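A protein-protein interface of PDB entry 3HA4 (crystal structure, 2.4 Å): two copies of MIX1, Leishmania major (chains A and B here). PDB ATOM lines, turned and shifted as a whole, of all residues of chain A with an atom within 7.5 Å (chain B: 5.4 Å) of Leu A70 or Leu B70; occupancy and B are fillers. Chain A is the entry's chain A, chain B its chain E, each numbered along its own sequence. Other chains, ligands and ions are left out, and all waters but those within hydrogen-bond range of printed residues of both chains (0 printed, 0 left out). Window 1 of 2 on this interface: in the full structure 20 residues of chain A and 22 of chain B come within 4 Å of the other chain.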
ATOM      1  N   TRP A  34     -28.855 -35.586  32.594  1.00  0.00           N
ATOM      2  CA  TRP A  34     -28.721 -34.692  31.446  1.00  0.00           C
ATOM      3  C   TRP A  34     -30.065 -34.305  30.781  1.00  0.00           C
ATOM      4  O   TRP A  34     -30.268 -33.143  30.427  1.00  0.00           O
ATOM      5  CB  TRP A  34     -27.714 -35.277  30.436  1.00  0.00           C
ATOM      6  CG  TRP A  34     -27.493 -34.430  29.212  1.00  0.00           C
ATOM      7  CD1 TRP A  34     -26.580 -33.422  29.060  1.00  0.00           C
ATOM      8  CD2 TRP A  34     -28.218 -34.506  27.975  1.00  0.00           C
ATOM      9  NE1 TRP A  34     -26.689 -32.871  27.807  1.00  0.00           N
ATOM     10  CE2 TRP A  34     -27.681 -33.518  27.118  1.00  0.00           C
ATOM     11  CE3 TRP A  34     -29.262 -35.316  27.508  1.00  0.00           C
ATOM     12  CZ2 TRP A  34     -28.155 -33.316  25.815  1.00  0.00           C
ATOM     13  CZ3 TRP A  34     -29.733 -35.116  26.212  1.00  0.00           C
ATOM     14  CH2 TRP A  34     -29.178 -34.122  25.383  1.00  0.00           C
ATOM     15  N   HIS A  38     -31.242 -30.547  30.334  1.00  0.00           N
ATOM     16  CA  HIS A  38     -31.498 -29.996  29.048  1.00  0.00           C
ATOM     17  C   HIS A  38     -32.885 -29.406  29.006  1.00  0.00           C
ATOM     18  O   HIS A  38     -33.089 -28.358  28.496  1.00  0.00           O
ATOM     19  CB  HIS A  38     -31.319 -31.050  27.984  1.00  0.00           C
ATOM     20  CG  HIS A  38     -31.772 -30.618  26.635  1.00  0.00           C
ATOM     21  ND1 HIS A  38     -33.072 -30.721  26.226  1.00  0.00           N
ATOM     22  CD2 HIS A  38     -31.100 -30.079  25.603  1.00  0.00           C
ATOM     23  CE1 HIS A  38     -33.182 -30.265  25.002  1.00  0.00           C
ATOM     24  NE2 HIS A  38     -32.001 -29.871  24.601  1.00  0.00           N
ATOM     25  N   VAL A  41     -32.984 -26.073  30.853  1.00  0.00           N
ATOM     26  CA  VAL A  41     -32.291 -25.036  30.138  1.00  0.00           C
ATOM     27  C   VAL A  41     -33.112 -24.539  28.976  1.00  0.00           C
ATOM     28  O   VAL A  41     -33.040 -23.408  28.603  1.00  0.00           O
ATOM     29  CB  VAL A  41     -30.943 -25.538  29.641  1.00  0.00           C
ATOM     30  CG1 VAL A  41     -30.389 -24.644  28.614  1.00  0.00           C
ATOM     31  CG2 VAL A  41     -29.997 -25.676  30.759  1.00  0.00           C
ATOM     32  N   VAL A  42     -33.923 -25.413  28.431  1.00  0.00           N
ATOM     33  CA  VAL A  42     -34.747 -25.082  27.308  1.00  0.00           C
ATOM     34  C   VAL A  42     -35.955 -24.237  27.647  1.00  0.00           C
ATOM     35  O   VAL A  42     -36.503 -23.615  26.792  1.00  0.00           O
ATOM     36  CB  VAL A  42     -35.174 -26.315  26.566  1.00  0.00           C
ATOM     37  CG1 VAL A  42     -36.210 -25.992  25.639  1.00  0.00           C
ATOM     38  CG2 VAL A  42     -34.060 -26.892  25.860  1.00  0.00           C
ATOM     39  N   ALA A  67     -18.319 -32.599  27.810  1.00  0.00           N
ATOM     40  CA  ALA A  67     -18.238 -33.010  26.408  1.00  0.00           C
ATOM     41  C   ALA A  67     -19.497 -32.728  25.605  1.00  0.00           C
ATOM     42  O   ALA A  67     -19.501 -32.923  24.391  1.00  0.00           O
ATOM     43  CB  ALA A  67     -17.869 -34.478  26.287  1.00  0.00           C
ATOM     44  N   ASP A  68     -20.558 -32.270  26.265  1.00  0.00           N
ATOM     45  CA  ASP A  68     -21.819 -31.995  25.574  1.00  0.00           C
ATOM     46  C   ASP A  68     -21.809 -30.677  24.790  1.00  0.00           C
ATOM     47  O   ASP A  68     -21.228 -29.675  25.233  1.00  0.00           O
ATOM     48  CB  ASP A  68     -22.985 -31.970  26.562  1.00  0.00           C
ATOM     49  CG  ASP A  68     -24.329 -31.782  25.869  1.00  0.00           C
ATOM     50  OD1 ASP A  68     -24.568 -32.467  24.842  1.00  0.00           O
ATOM     51  OD2 ASP A  68     -25.136 -30.948  26.343  1.00  0.00           O
ATOM     52  N   TRP A  69     -22.476 -30.674  23.638  1.00  0.00           N
ATOM     53  CA  TRP A  69     -22.571 -29.459  22.808  1.00  0.00           C
ATOM     54  C   TRP A  69     -24.002 -28.920  22.795  1.00  0.00           C
ATOM     55  O   TRP A  69     -24.221 -27.733  22.560  1.00  0.00           O
ATOM     56  CB  TRP A  69     -22.092 -29.722  21.357  1.00  0.00           C
ATOM     57  CG  TRP A  69     -22.846 -30.836  20.728  1.00  0.00           C
ATOM     58  CD1 TRP A  69     -22.571 -32.163  20.829  1.00  0.00           C
ATOM     59  CD2 TRP A  69     -24.052 -30.733  19.965  1.00  0.00           C
ATOM     60  NE1 TRP A  69     -23.522 -32.896  20.161  1.00  0.00           N
ATOM     61  CE2 TRP A  69     -24.441 -32.039  19.618  1.00  0.00           C
ATOM     62  CE3 TRP A  69     -24.831 -29.663  19.526  1.00  0.00           C
ATOM     63  CZ2 TRP A  69     -25.566 -32.303  18.848  1.00  0.00           C
ATOM     64  CZ3 TRP A  69     -25.952 -29.929  18.769  1.00  0.00           C
ATOM     65  CH2 TRP A  69     -26.306 -31.237  18.432  1.00  0.00           C
ATOM     66  N   LEU A  70     -24.968 -29.802  23.040  1.00  0.00           N
ATOM     67  CA  LEU A  70     -26.380 -29.450  22.926  1.00  0.00           C
ATOM     68  C   LEU A  70     -26.782 -28.364  23.917  1.00  0.00           C
ATOM     69  O   LEU A  70     -27.384 -27.352  23.552  1.00  0.00           O
ATOM     70  CB  LEU A  70     -27.260 -30.688  23.112  1.00  0.00           C
ATOM     71  CG  LEU A  70     -28.737 -30.530  22.743  1.00  0.00           C
ATOM     72  CD1 LEU A  70     -28.906 -29.677  21.486  1.00  0.00           C
ATOM     73  CD2 LEU A  70     -29.392 -31.887  22.555  1.00  0.00           C
ATOM     74  N   ILE A  71     -26.438 -28.567  25.179  1.00  0.00           N
ATOM     75  CA  ILE A  71     -26.777 -27.585  26.186  1.00  0.00           C
ATOM     76  C   ILE A  71     -26.054 -26.257  25.937  1.00  0.00           C
ATOM     77  O   ILE A  71     -26.677 -25.197  25.995  1.00  0.00           O
ATOM     78  CB  ILE A  71     -26.571 -28.147  27.608  1.00  0.00           C
ATOM     79  CG1 ILE A  71     -27.666 -29.182  27.891  1.00  0.00           C
ATOM     80  CG2 ILE A  71     -26.576 -27.016  28.647  1.00  0.00           C
ATOM     81  CD1 ILE A  71     -27.624 -29.808  29.271  1.00  0.00           C
ATOM     82  N   PRO A  72     -24.742 -26.306  25.633  1.00  0.00           N
ATOM     83  CA  PRO A  72     -24.034 -25.065  25.272  1.00  0.00           C
ATOM     84  C   PRO A  72     -24.642 -24.347  24.068  1.00  0.00           C
ATOM     85  O   PRO A  72     -24.673 -23.116  24.038  1.00  0.00           O
ATOM     86  CB  PRO A  72     -22.621 -25.551  24.961  1.00  0.00           C
ATOM     87  CG  PRO A  72     -22.464 -26.747  25.855  1.00  0.00           C
ATOM     88  CD  PRO A  72     -23.808 -27.427  25.835  1.00  0.00           C
ATOM     89  N   LEU A  73     -25.121 -25.109  23.092  1.00  0.00           N
ATOM     90  CA  LEU A  73     -25.836 -24.533  21.966  1.00  0.00           C
ATOM     91  C   LEU A  73     -27.081 -23.774  22.457  1.00  0.00           C
ATOM     92  O   LEU A  73     -27.325 -22.630  22.071  1.00  0.00           O
ATOM     93  CB  LEU A  73     -26.232 -25.640  20.984  1.00  0.00           C
ATOM     94  CG  LEU A  73     -26.954 -25.245  19.697  1.00  0.00           C
ATOM     95  CD1 LEU A  73     -26.003 -24.503  18.791  1.00  0.00           C
ATOM     96  CD2 LEU A  73     -27.510 -26.476  19.010  1.00  0.00           C
ATOM     97  N   GLU A  74     -27.854 -24.411  23.328  1.00  0.00           N
ATOM     98  CA  GLU A  74     -29.064 -23.800  23.879  1.00  0.00           C
ATOM     99  C   GLU A  74     -28.745 -22.551  24.717  1.00  0.00           C
ATOM    100  O   GLU A  74     -29.389 -21.507  24.570  1.00  0.00           O
ATOM    101  CB  GLU A  74     -29.835 -24.827  24.695  1.00  0.00           C
ATOM    102  CG  GLU A  74     -31.323 -24.611  24.693  1.00  0.00           C
ATOM    103  CD  GLU A  74     -31.898 -24.658  23.293  1.00  0.00           C
ATOM    104  OE1 GLU A  74     -32.162 -25.770  22.762  1.00  0.00           O
ATOM    105  OE2 GLU A  74     -32.085 -23.565  22.726  1.00  0.00           O
ATOM    106  N   LEU A  75     -27.741 -22.656  25.582  1.00  0.00           N
ATOM    107  CA  LEU A  75     -27.252 -21.502  26.325  1.00  0.00           C
ATOM    108  C   LEU A  75     -26.794 -20.356  25.415  1.00  0.00           C
ATOM    109  O   LEU A  75     -27.004 -19.179  25.733  1.00  0.00           O
ATOM    110  CB  LEU A  75     -26.114 -21.925  27.255  1.00  0.00           C
ATOM    111  CG  LEU A  75     -26.422 -22.225  28.721  1.00  0.00           C
ATOM    112  CD1 LEU A  75     -27.908 -22.197  29.011  1.00  0.00           C
ATOM    113  CD2 LEU A  75     -25.818 -23.547  29.104  1.00  0.00           C
ATOM    114  N   THR A  76     -26.165 -20.693  24.287  1.00  0.00           N
ATOM    115  CA  THR A  76     -25.757 -19.673  23.331  1.00  0.00           C
ATOM    116  C   THR A  76     -26.967 -18.869  22.860  1.00  0.00           C
ATOM    117  O   THR A  76     -26.908 -17.644  22.790  1.00  0.00           O
ATOM    118  CB  THR A  76     -25.040 -20.265  22.107  1.00  0.00           C
ATOM    119  OG1 THR A  76     -23.838 -20.910  22.525  1.00  0.00           O
ATOM    120  CG2 THR A  76     -24.684 -19.166  21.125  1.00  0.00           C
ATOM    121  N   GLN A 104     -16.146 -24.612  25.981  1.00  0.00           N
ATOM    122  CA  GLN A 104     -16.628 -25.994  25.932  1.00  0.00           C
ATOM    123  C   GLN A 104     -16.999 -26.449  24.513  1.00  0.00           C
ATOM    124  O   GLN A 104     -16.713 -27.584  24.130  1.00  0.00           O
ATOM    125  CB  GLN A 104     -17.780 -26.238  26.900  1.00  0.00           C
ATOM    126  CG  GLN A 104     -18.523 -27.533  26.620  1.00  0.00           C
ATOM    127  CD  GLN A 104     -19.199 -28.100  27.847  1.00  0.00           C
ATOM    128  OE1 GLN A 104     -18.812 -27.803  28.970  1.00  0.00           O
ATOM    129  NE2 GLN A 104     -20.201 -28.934  27.637  1.00  0.00           N
ATOM    130  N   LEU A 105     -17.639 -25.564  23.748  1.00  0.00           N
ATOM    131  CA  LEU A 105     -17.991 -25.866  22.362  1.00  0.00           C
ATOM    132  C   LEU A 105     -16.723 -26.103  21.556  1.00  0.00           C
ATOM    133  O   LEU A 105     -16.668 -27.015  20.740  1.00  0.00           O
ATOM    134  CB  LEU A 105     -18.841 -24.753  21.736  1.00  0.00           C
ATOM    135  CG  LEU A 105     -20.323 -24.776  22.139  1.00  0.00           C
ATOM    136  CD1 LEU A 105     -21.035 -23.511  21.704  1.00  0.00           C
ATOM    137  CD2 LEU A 105     -20.979 -25.983  21.549  1.00  0.00           C
ATOM    138  N   VAL A 108     -15.307 -29.515  22.216  1.00  0.00           N
ATOM    139  CA  VAL A 108     -16.042 -30.565  21.508  1.00  0.00           C
ATOM    140  C   VAL A 108     -15.668 -30.601  20.024  1.00  0.00           C
ATOM    141  O   VAL A 108     -15.462 -31.663  19.443  1.00  0.00           O
ATOM    142  CB  VAL A 108     -17.562 -30.364  21.622  1.00  0.00           C
ATOM    143  CG1 VAL A 108     -18.294 -31.319  20.695  1.00  0.00           C
ATOM    144  CG2 VAL A 108     -18.021 -30.539  23.080  1.00  0.00           C
ATOM    145  N   PRO A 116     -19.978 -36.688  23.549  1.00  0.00           N
ATOM    146  CA  PRO A 116     -20.984 -35.657  23.758  1.00  0.00           C
ATOM    147  C   PRO A 116     -22.376 -36.191  23.859  1.00  0.00           C
ATOM    148  O   PRO A 116     -22.787 -37.039  23.114  1.00  0.00           O
ATOM    149  CB  PRO A 116     -20.849 -34.805  22.508  1.00  0.00           C
ATOM    150  CG  PRO A 116     -19.497 -35.030  22.061  1.00  0.00           C
ATOM    151  CD  PRO A 116     -19.264 -36.455  22.291  1.00  0.00           C
ATOM    152  N   ASN A 117     -23.095 -35.642  24.813  1.00  0.00           N
ATOM    153  CA  ASN A 117     -24.430 -36.057  25.158  1.00  0.00           C
ATOM    154  C   ASN A 117     -25.398 -35.850  24.046  1.00  0.00           C
ATOM    155  O   ASN A 117     -26.322 -36.597  23.900  1.00  0.00           O
ATOM    156  CB  ASN A 117     -24.894 -35.349  26.409  1.00  0.00           C
ATOM    157  CG  ASN A 117     -24.048 -35.676  27.584  1.00  0.00           C
ATOM    158  OD1 ASN A 117     -22.962 -35.191  27.721  1.00  0.00           O
ATOM    159  ND2 ASN A 117     -24.542 -36.542  28.426  1.00  0.00           N
ATOM    160  N   GLY A 118     -25.191 -34.800  23.280  1.00  0.00           N
ATOM    161  CA  GLY A 118     -26.099 -34.437  22.218  1.00  0.00           C
ATOM    162  C   GLY A 118     -26.016 -35.430  21.093  1.00  0.00           C
ATOM    163  O   GLY A 118     -26.744 -35.363  20.125  1.00  0.00           O
ATOM    164  N   GLY A 119     -25.051 -36.319  21.192  1.00  0.00           N
ATOM    165  CA  GLY A 119     -24.761 -37.222  20.124  1.00  0.00           C
ATOM    166  C   GLY A 119     -23.490 -36.902  19.398  1.00  0.00           C
ATOM    167  O   GLY A 119     -22.794 -35.969  19.693  1.00  0.00           O
ATOM    168  N   VAL A 125     -22.962 -31.596  12.837  1.00  0.00           N
ATOM    169  CA  VAL A 125     -22.948 -31.151  14.189  1.00  0.00           C
ATOM    170  C   VAL A 125     -21.777 -30.258  14.397  1.00  0.00           C
ATOM    171  O   VAL A 125     -21.862 -29.340  15.143  1.00  0.00           O
ATOM    172  CB  VAL A 125     -22.824 -32.299  15.142  1.00  0.00           C
ATOM    173  CG1 VAL A 125     -22.355 -31.830  16.409  1.00  0.00           C
ATOM    174  CG2 VAL A 125     -24.111 -32.952  15.318  1.00  0.00           C
ATOM    175  N   ILE A 128     -22.822 -26.774  13.063  1.00  0.00           N
ATOM    176  CA  ILE A 128     -23.731 -26.061  13.920  1.00  0.00           C
ATOM    177  C   ILE A 128     -23.030 -25.479  15.135  1.00  0.00           C
ATOM    178  O   ILE A 128     -23.417 -24.458  15.623  1.00  0.00           O
ATOM    179  CB  ILE A 128     -24.907 -26.963  14.291  1.00  0.00           C
ATOM    180  CG1 ILE A 128     -26.164 -26.158  14.435  1.00  0.00           C
ATOM    181  CG2 ILE A 128     -24.666 -27.711  15.525  1.00  0.00           C
ATOM    182  CD1 ILE A 128     -27.276 -26.927  14.916  1.00  0.00           C
ATOM    183  N   ILE A 129     -21.982 -26.151  15.570  1.00  0.00           N
ATOM    184  CA  ILE A 129     -21.107 -25.738  16.619  1.00  0.00           C
ATOM    185  C   ILE A 129     -20.204 -24.633  16.173  1.00  0.00           C
ATOM    186  O   ILE A 129     -19.884 -23.772  16.919  1.00  0.00           O
ATOM    187  CB  ILE A 129     -20.262 -26.923  17.079  1.00  0.00           C
ATOM    188  CG1 ILE A 129     -21.129 -27.954  17.756  1.00  0.00           C
ATOM    189  CG2 ILE A 129     -19.184 -26.508  18.007  1.00  0.00           C
ATOM    190  CD1 ILE A 129     -20.414 -29.111  18.158  1.00  0.00           C
ATOM    191  N   TRP B  34     -27.930 -27.440   7.232  1.00  0.00           N
ATOM    192  CA  TRP B  34     -28.559 -27.739   8.497  1.00  0.00           C
ATOM    193  C   TRP B  34     -28.453 -26.651   9.539  1.00  0.00           C
ATOM    194  O   TRP B  34     -29.422 -26.301  10.175  1.00  0.00           O
ATOM    195  CB  TRP B  34     -27.953 -29.025   9.039  1.00  0.00           C
ATOM    196  CG  TRP B  34     -28.719 -29.639  10.131  1.00  0.00           C
ATOM    197  CD1 TRP B  34     -29.997 -30.000  10.098  1.00  0.00           C
ATOM    198  CD2 TRP B  34     -28.241 -29.967  11.415  1.00  0.00           C
ATOM    199  NE1 TRP B  34     -30.369 -30.540  11.266  1.00  0.00           N
ATOM    200  CE2 TRP B  34     -29.298 -30.523  12.108  1.00  0.00           C
ATOM    201  CE3 TRP B  34     -27.017 -29.831  12.058  1.00  0.00           C
ATOM    202  CZ2 TRP B  34     -29.180 -30.946  13.401  1.00  0.00           C
ATOM    203  CZ3 TRP B  34     -26.904 -30.251  13.307  1.00  0.00           C
ATOM    204  CH2 TRP B  34     -27.971 -30.807  13.980  1.00  0.00           C
ATOM    205  N   HIS B  38     -31.540 -24.767  10.905  1.00  0.00           N
ATOM    206  CA  HIS B  38     -31.767 -24.754  12.344  1.00  0.00           C
ATOM    207  C   HIS B  38     -31.817 -23.319  12.858  1.00  0.00           C
ATOM    208  O   HIS B  38     -32.664 -22.973  13.683  1.00  0.00           O
ATOM    209  CB  HIS B  38     -30.670 -25.535  13.068  1.00  0.00           C
ATOM    210  CG  HIS B  38     -30.712 -25.397  14.559  1.00  0.00           C
ATOM    211  ND1 HIS B  38     -29.930 -24.494  15.244  1.00  0.00           N
ATOM    212  CD2 HIS B  38     -31.441 -26.049  15.493  1.00  0.00           C
ATOM    213  CE1 HIS B  38     -30.177 -24.594  16.538  1.00  0.00           C
ATOM    214  NE2 HIS B  38     -31.091 -25.531  16.716  1.00  0.00           N
ATOM    215  N   ASP B  68     -33.463 -36.017  11.451  1.00  0.00           N
ATOM    216  CA  ASP B  68     -33.005 -35.086  12.467  1.00  0.00           C
ATOM    217  C   ASP B  68     -34.047 -34.938  13.556  1.00  0.00           C
ATOM    218  O   ASP B  68     -35.242 -34.955  13.279  1.00  0.00           O
ATOM    219  CB  ASP B  68     -32.673 -33.718  11.873  1.00  0.00           C
ATOM    220  CG  ASP B  68     -32.253 -32.709  12.937  1.00  0.00           C
ATOM    221  OD1 ASP B  68     -31.441 -33.075  13.823  1.00  0.00           O
ATOM    222  OD2 ASP B  68     -32.742 -31.556  12.891  1.00  0.00           O
ATOM    223  N   TRP B  69     -33.587 -34.797  14.795  1.00  0.00           N
ATOM    224  CA  TRP B  69     -34.486 -34.555  15.919  1.00  0.00           C
ATOM    225  C   TRP B  69     -34.348 -33.121  16.388  1.00  0.00           C
ATOM    226  O   TRP B  69     -35.278 -32.553  16.950  1.00  0.00           O
ATOM    227  CB  TRP B  69     -34.181 -35.505  17.078  1.00  0.00           C
ATOM    228  CG  TRP B  69     -32.712 -35.617  17.389  1.00  0.00           C
ATOM    229  CD1 TRP B  69     -31.841 -36.553  16.906  1.00  0.00           C
ATOM    230  CD2 TRP B  69     -31.946 -34.762  18.246  1.00  0.00           C
ATOM    231  NE1 TRP B  69     -30.582 -36.332  17.410  1.00  0.00           N
ATOM    232  CE2 TRP B  69     -30.617 -35.240  18.235  1.00  0.00           C
ATOM    233  CE3 TRP B  69     -32.253 -33.636  19.019  1.00  0.00           C
ATOM    234  CZ2 TRP B  69     -29.595 -34.633  18.972  1.00  0.00           C
ATOM    235  CZ3 TRP B  69     -31.236 -33.034  19.748  1.00  0.00           C
ATOM    236  CH2 TRP B  69     -29.924 -33.535  19.716  1.00  0.00           C
ATOM    237  N   LEU B  70     -33.180 -32.542  16.142  1.00  0.00           N
ATOM    238  CA  LEU B  70     -32.864 -31.219  16.651  1.00  0.00           C
ATOM    239  C   LEU B  70     -33.912 -30.208  16.231  1.00  0.00           C
ATOM    240  O   LEU B  70     -34.465 -29.475  17.060  1.00  0.00           O
ATOM    241  CB  LEU B  70     -31.497 -30.767  16.143  1.00  0.00           C
ATOM    242  CG  LEU B  70     -31.101 -29.425  16.746  1.00  0.00           C
ATOM    243  CD1 LEU B  70     -31.018 -29.574  18.259  1.00  0.00           C
ATOM    244  CD2 LEU B  70     -29.792 -28.924  16.162  1.00  0.00           C
ATOM    245  N   ILE B  71     -34.174 -30.163  14.928  1.00  0.00           N
ATOM    246  CA  ILE B  71     -35.136 -29.216  14.390  1.00  0.00           C
ATOM    247  C   ILE B  71     -36.553 -29.509  14.895  1.00  0.00           C
ATOM    248  O   ILE B  71     -37.248 -28.599  15.359  1.00  0.00           O
ATOM    249  CB  ILE B  71     -35.059 -29.138  12.852  1.00  0.00           C
ATOM    250  CG1 ILE B  71     -33.708 -28.546  12.449  1.00  0.00           C
ATOM    251  CG2 ILE B  71     -36.201 -28.297  12.305  1.00  0.00           C
ATOM    252  CD1 ILE B  71     -33.387 -28.652  10.994  1.00  0.00           C
ATOM    253  N   PRO B  72     -36.983 -30.780  14.828  1.00  0.00           N
ATOM    254  CA  PRO B  72     -38.292 -31.113  15.391  1.00  0.00           C
ATOM    255  C   PRO B  72     -38.471 -30.633  16.838  1.00  0.00           C
ATOM    256  O   PRO B  72     -39.543 -30.115  17.170  1.00  0.00           O
ATOM    257  CB  PRO B  72     -38.320 -32.635  15.303  1.00  0.00           C
ATOM    258  CG  PRO B  72     -37.503 -32.940  14.120  1.00  0.00           C
ATOM    259  CD  PRO B  72     -36.414 -31.905  14.067  1.00  0.00           C
ATOM    260  N   LEU B  73     -37.445 -30.785  17.676  1.00  0.00           N
ATOM    261  CA  LEU B  73     -37.509 -30.283  19.058  1.00  0.00           C
ATOM    262  C   LEU B  73     -37.722 -28.772  19.123  1.00  0.00           C
ATOM    263  O   LEU B  73     -38.531 -28.296  19.922  1.00  0.00           O
ATOM    264  CB  LEU B  73     -36.279 -30.689  19.895  1.00  0.00           C
ATOM    265  CG  LEU B  73     -36.423 -31.955  20.751  1.00  0.00           C
ATOM    266  CD1 LEU B  73     -36.877 -33.139  19.907  1.00  0.00           C
ATOM    267  CD2 LEU B  73     -35.130 -32.290  21.507  1.00  0.00           C
ATOM    268  N   GLU B  74     -37.011 -28.009  18.296  1.00  0.00           N
ATOM    269  CA  GLU B  74     -37.189 -26.566  18.351  1.00  0.00           C
ATOM    270  C   GLU B  74     -38.593 -26.198  17.922  1.00  0.00           C
ATOM    271  O   GLU B  74     -39.208 -25.279  18.481  1.00  0.00           O
ATOM    272  CB  GLU B  74     -36.195 -25.828  17.471  1.00  0.00           C
ATOM    273  CG  GLU B  74     -36.282 -24.318  17.683  1.00  0.00           C
ATOM    274  CD  GLU B  74     -35.749 -23.898  19.041  1.00  0.00           C
ATOM    275  OE1 GLU B  74     -34.930 -24.655  19.604  1.00  0.00           O
ATOM    276  OE2 GLU B  74     -36.140 -22.820  19.545  1.00  0.00           O
ATOM    277  N   LEU B  75     -39.084 -26.928  16.922  1.00  0.00           N
ATOM    278  CA  LEU B  75     -40.396 -26.706  16.337  1.00  0.00           C
ATOM    279  C   LEU B  75     -41.482 -26.978  17.368  1.00  0.00           C
ATOM    280  O   LEU B  75     -42.484 -26.256  17.450  1.00  0.00           O
ATOM    281  CB  LEU B  75     -40.581 -27.621  15.133  1.00  0.00           C
ATOM    282  CG  LEU B  75     -40.950 -26.908  13.836  1.00  0.00           C
ATOM    283  CD1 LEU B  75     -40.034 -25.718  13.609  1.00  0.00           C
ATOM    284  CD2 LEU B  75     -40.863 -27.876  12.673  1.00  0.00           C
ATOM    285  N   ILE B 128     -34.682 -36.941  25.631  1.00  0.00           N
ATOM    286  CA  ILE B 128     -35.186 -35.596  25.364  1.00  0.00           C
ATOM    287  C   ILE B 128     -36.140 -35.626  24.174  1.00  0.00           C
ATOM    288  O   ILE B 128     -37.070 -34.830  24.112  1.00  0.00           O
ATOM    289  CB  ILE B 128     -34.089 -34.500  25.224  1.00  0.00           C
ATOM    290  CG1 ILE B 128     -33.255 -34.684  23.960  1.00  0.00           C
ATOM    291  CG2 ILE B 128     -33.206 -34.452  26.467  1.00  0.00           C
ATOM    292  CD1 ILE B 128     -32.183 -33.658  23.843  1.00  0.00           C
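The indole nitrogen (NE1) of Trp A34 lies within hydrogen-bond range of the side-chain carboxylate (OD2) of Asp A68. The backbone NH (N) of Leu A70 lies within hydrogen-bond range of the side-chain carboxylate (OD1) of Asp A68 (3.2 Å). N of Gly A118 lies within hydrogen-bond range of OD1 of Asp A68, at 2.9 Å. The side-chain carboxylate of Asp B68 lies within hydrogen-bond range of the indole nitrogen of Trp B34 (3.1 Å). The side-chain carboxylate (OD1) of Asp B68 lies within hydrogen-bond range of the backbone NH (N) of Leu B70 (2.9 Å).
Trp A34 touches Ile B128. CE1 of His A38 touches CD1 of Ile B128, 3.7 Å away. Trp B69 touches Leu A70. CD1 of Leu A70 touches CD1 of Leu B70, at 3.9 Å. CD2 of Leu A70 touches CD1 of Ile B128, at 3.5 Å. Gly A118 touches Trp B69. CZ3 of Trp B34 touches CD1 of Ile A128, at 3.7 Å. Ile A128 touches His B38. Ile A128 touches Leu B70 (CD1 to CD2, 3.4 Å).
Of chain B, only Trp B69 (3.3 Å), Leu B70 (3.9 Å) and Ile B128 (3.5 Å) come within 4 Å of Leu A70. Printed residues of chain A within 4 Å of Leu B70: Leu A70 and Ile A128. Of the printed residues of chain B, His A38 touches Ile B128. Of the printed residues of chain B, Ile A128 touches Trp B34, His B38 and Leu B70. Of the printed residues of chain B, Gly A118 touches Trp B69. Of the printed residues of chain A, His B38 touches Ile A128. Printed residues of chain A within 4 Å of Ile B128: Trp A34 (3.4 Å), His A38 (3.7 Å) and Leu A70 (3.5 Å). Leu A73 touches none of the printed residues of chain B. The nearest residue of chain A that does not touch Leu B70 is Leu A73 (4.4 Å).
Of the 24 printed residues of chain A, 5 touch a printed residue of chain B. Printed residues of chain B that touch a printed residue of chain A: Trp B34, His B38, Trp B69, Leu B70 and Ile B128. Hydrophobic or aromatic side chains of chain B that line the printed part of chain A: Trp B34, His B38, Trp B69, Leu B70 and Ile B128. Among the printed residues, 9 pairs touch across the chains. Among the printed residues, no Asp or Glu carboxylate lies within 4 Å of a Lys or Arg side-chain nitrogen of the other chain.
Trp A34 touches Ile B128, and with the chains exchanged Ile A128 touches Trp B34. His A38 touches Ile B128, and with the chains exchanged Ile A128 touches His B38. Leu B70 touches its own counterpart, Leu A70. Leu A70 touches Ile B128, and with the chains exchanged Ile A128 touches Leu B70. 11 positions are printed for both chains. Of the 9 pairs that touch across the chains among the printed residues, 7 have their exchanged pair printed and touching as well.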
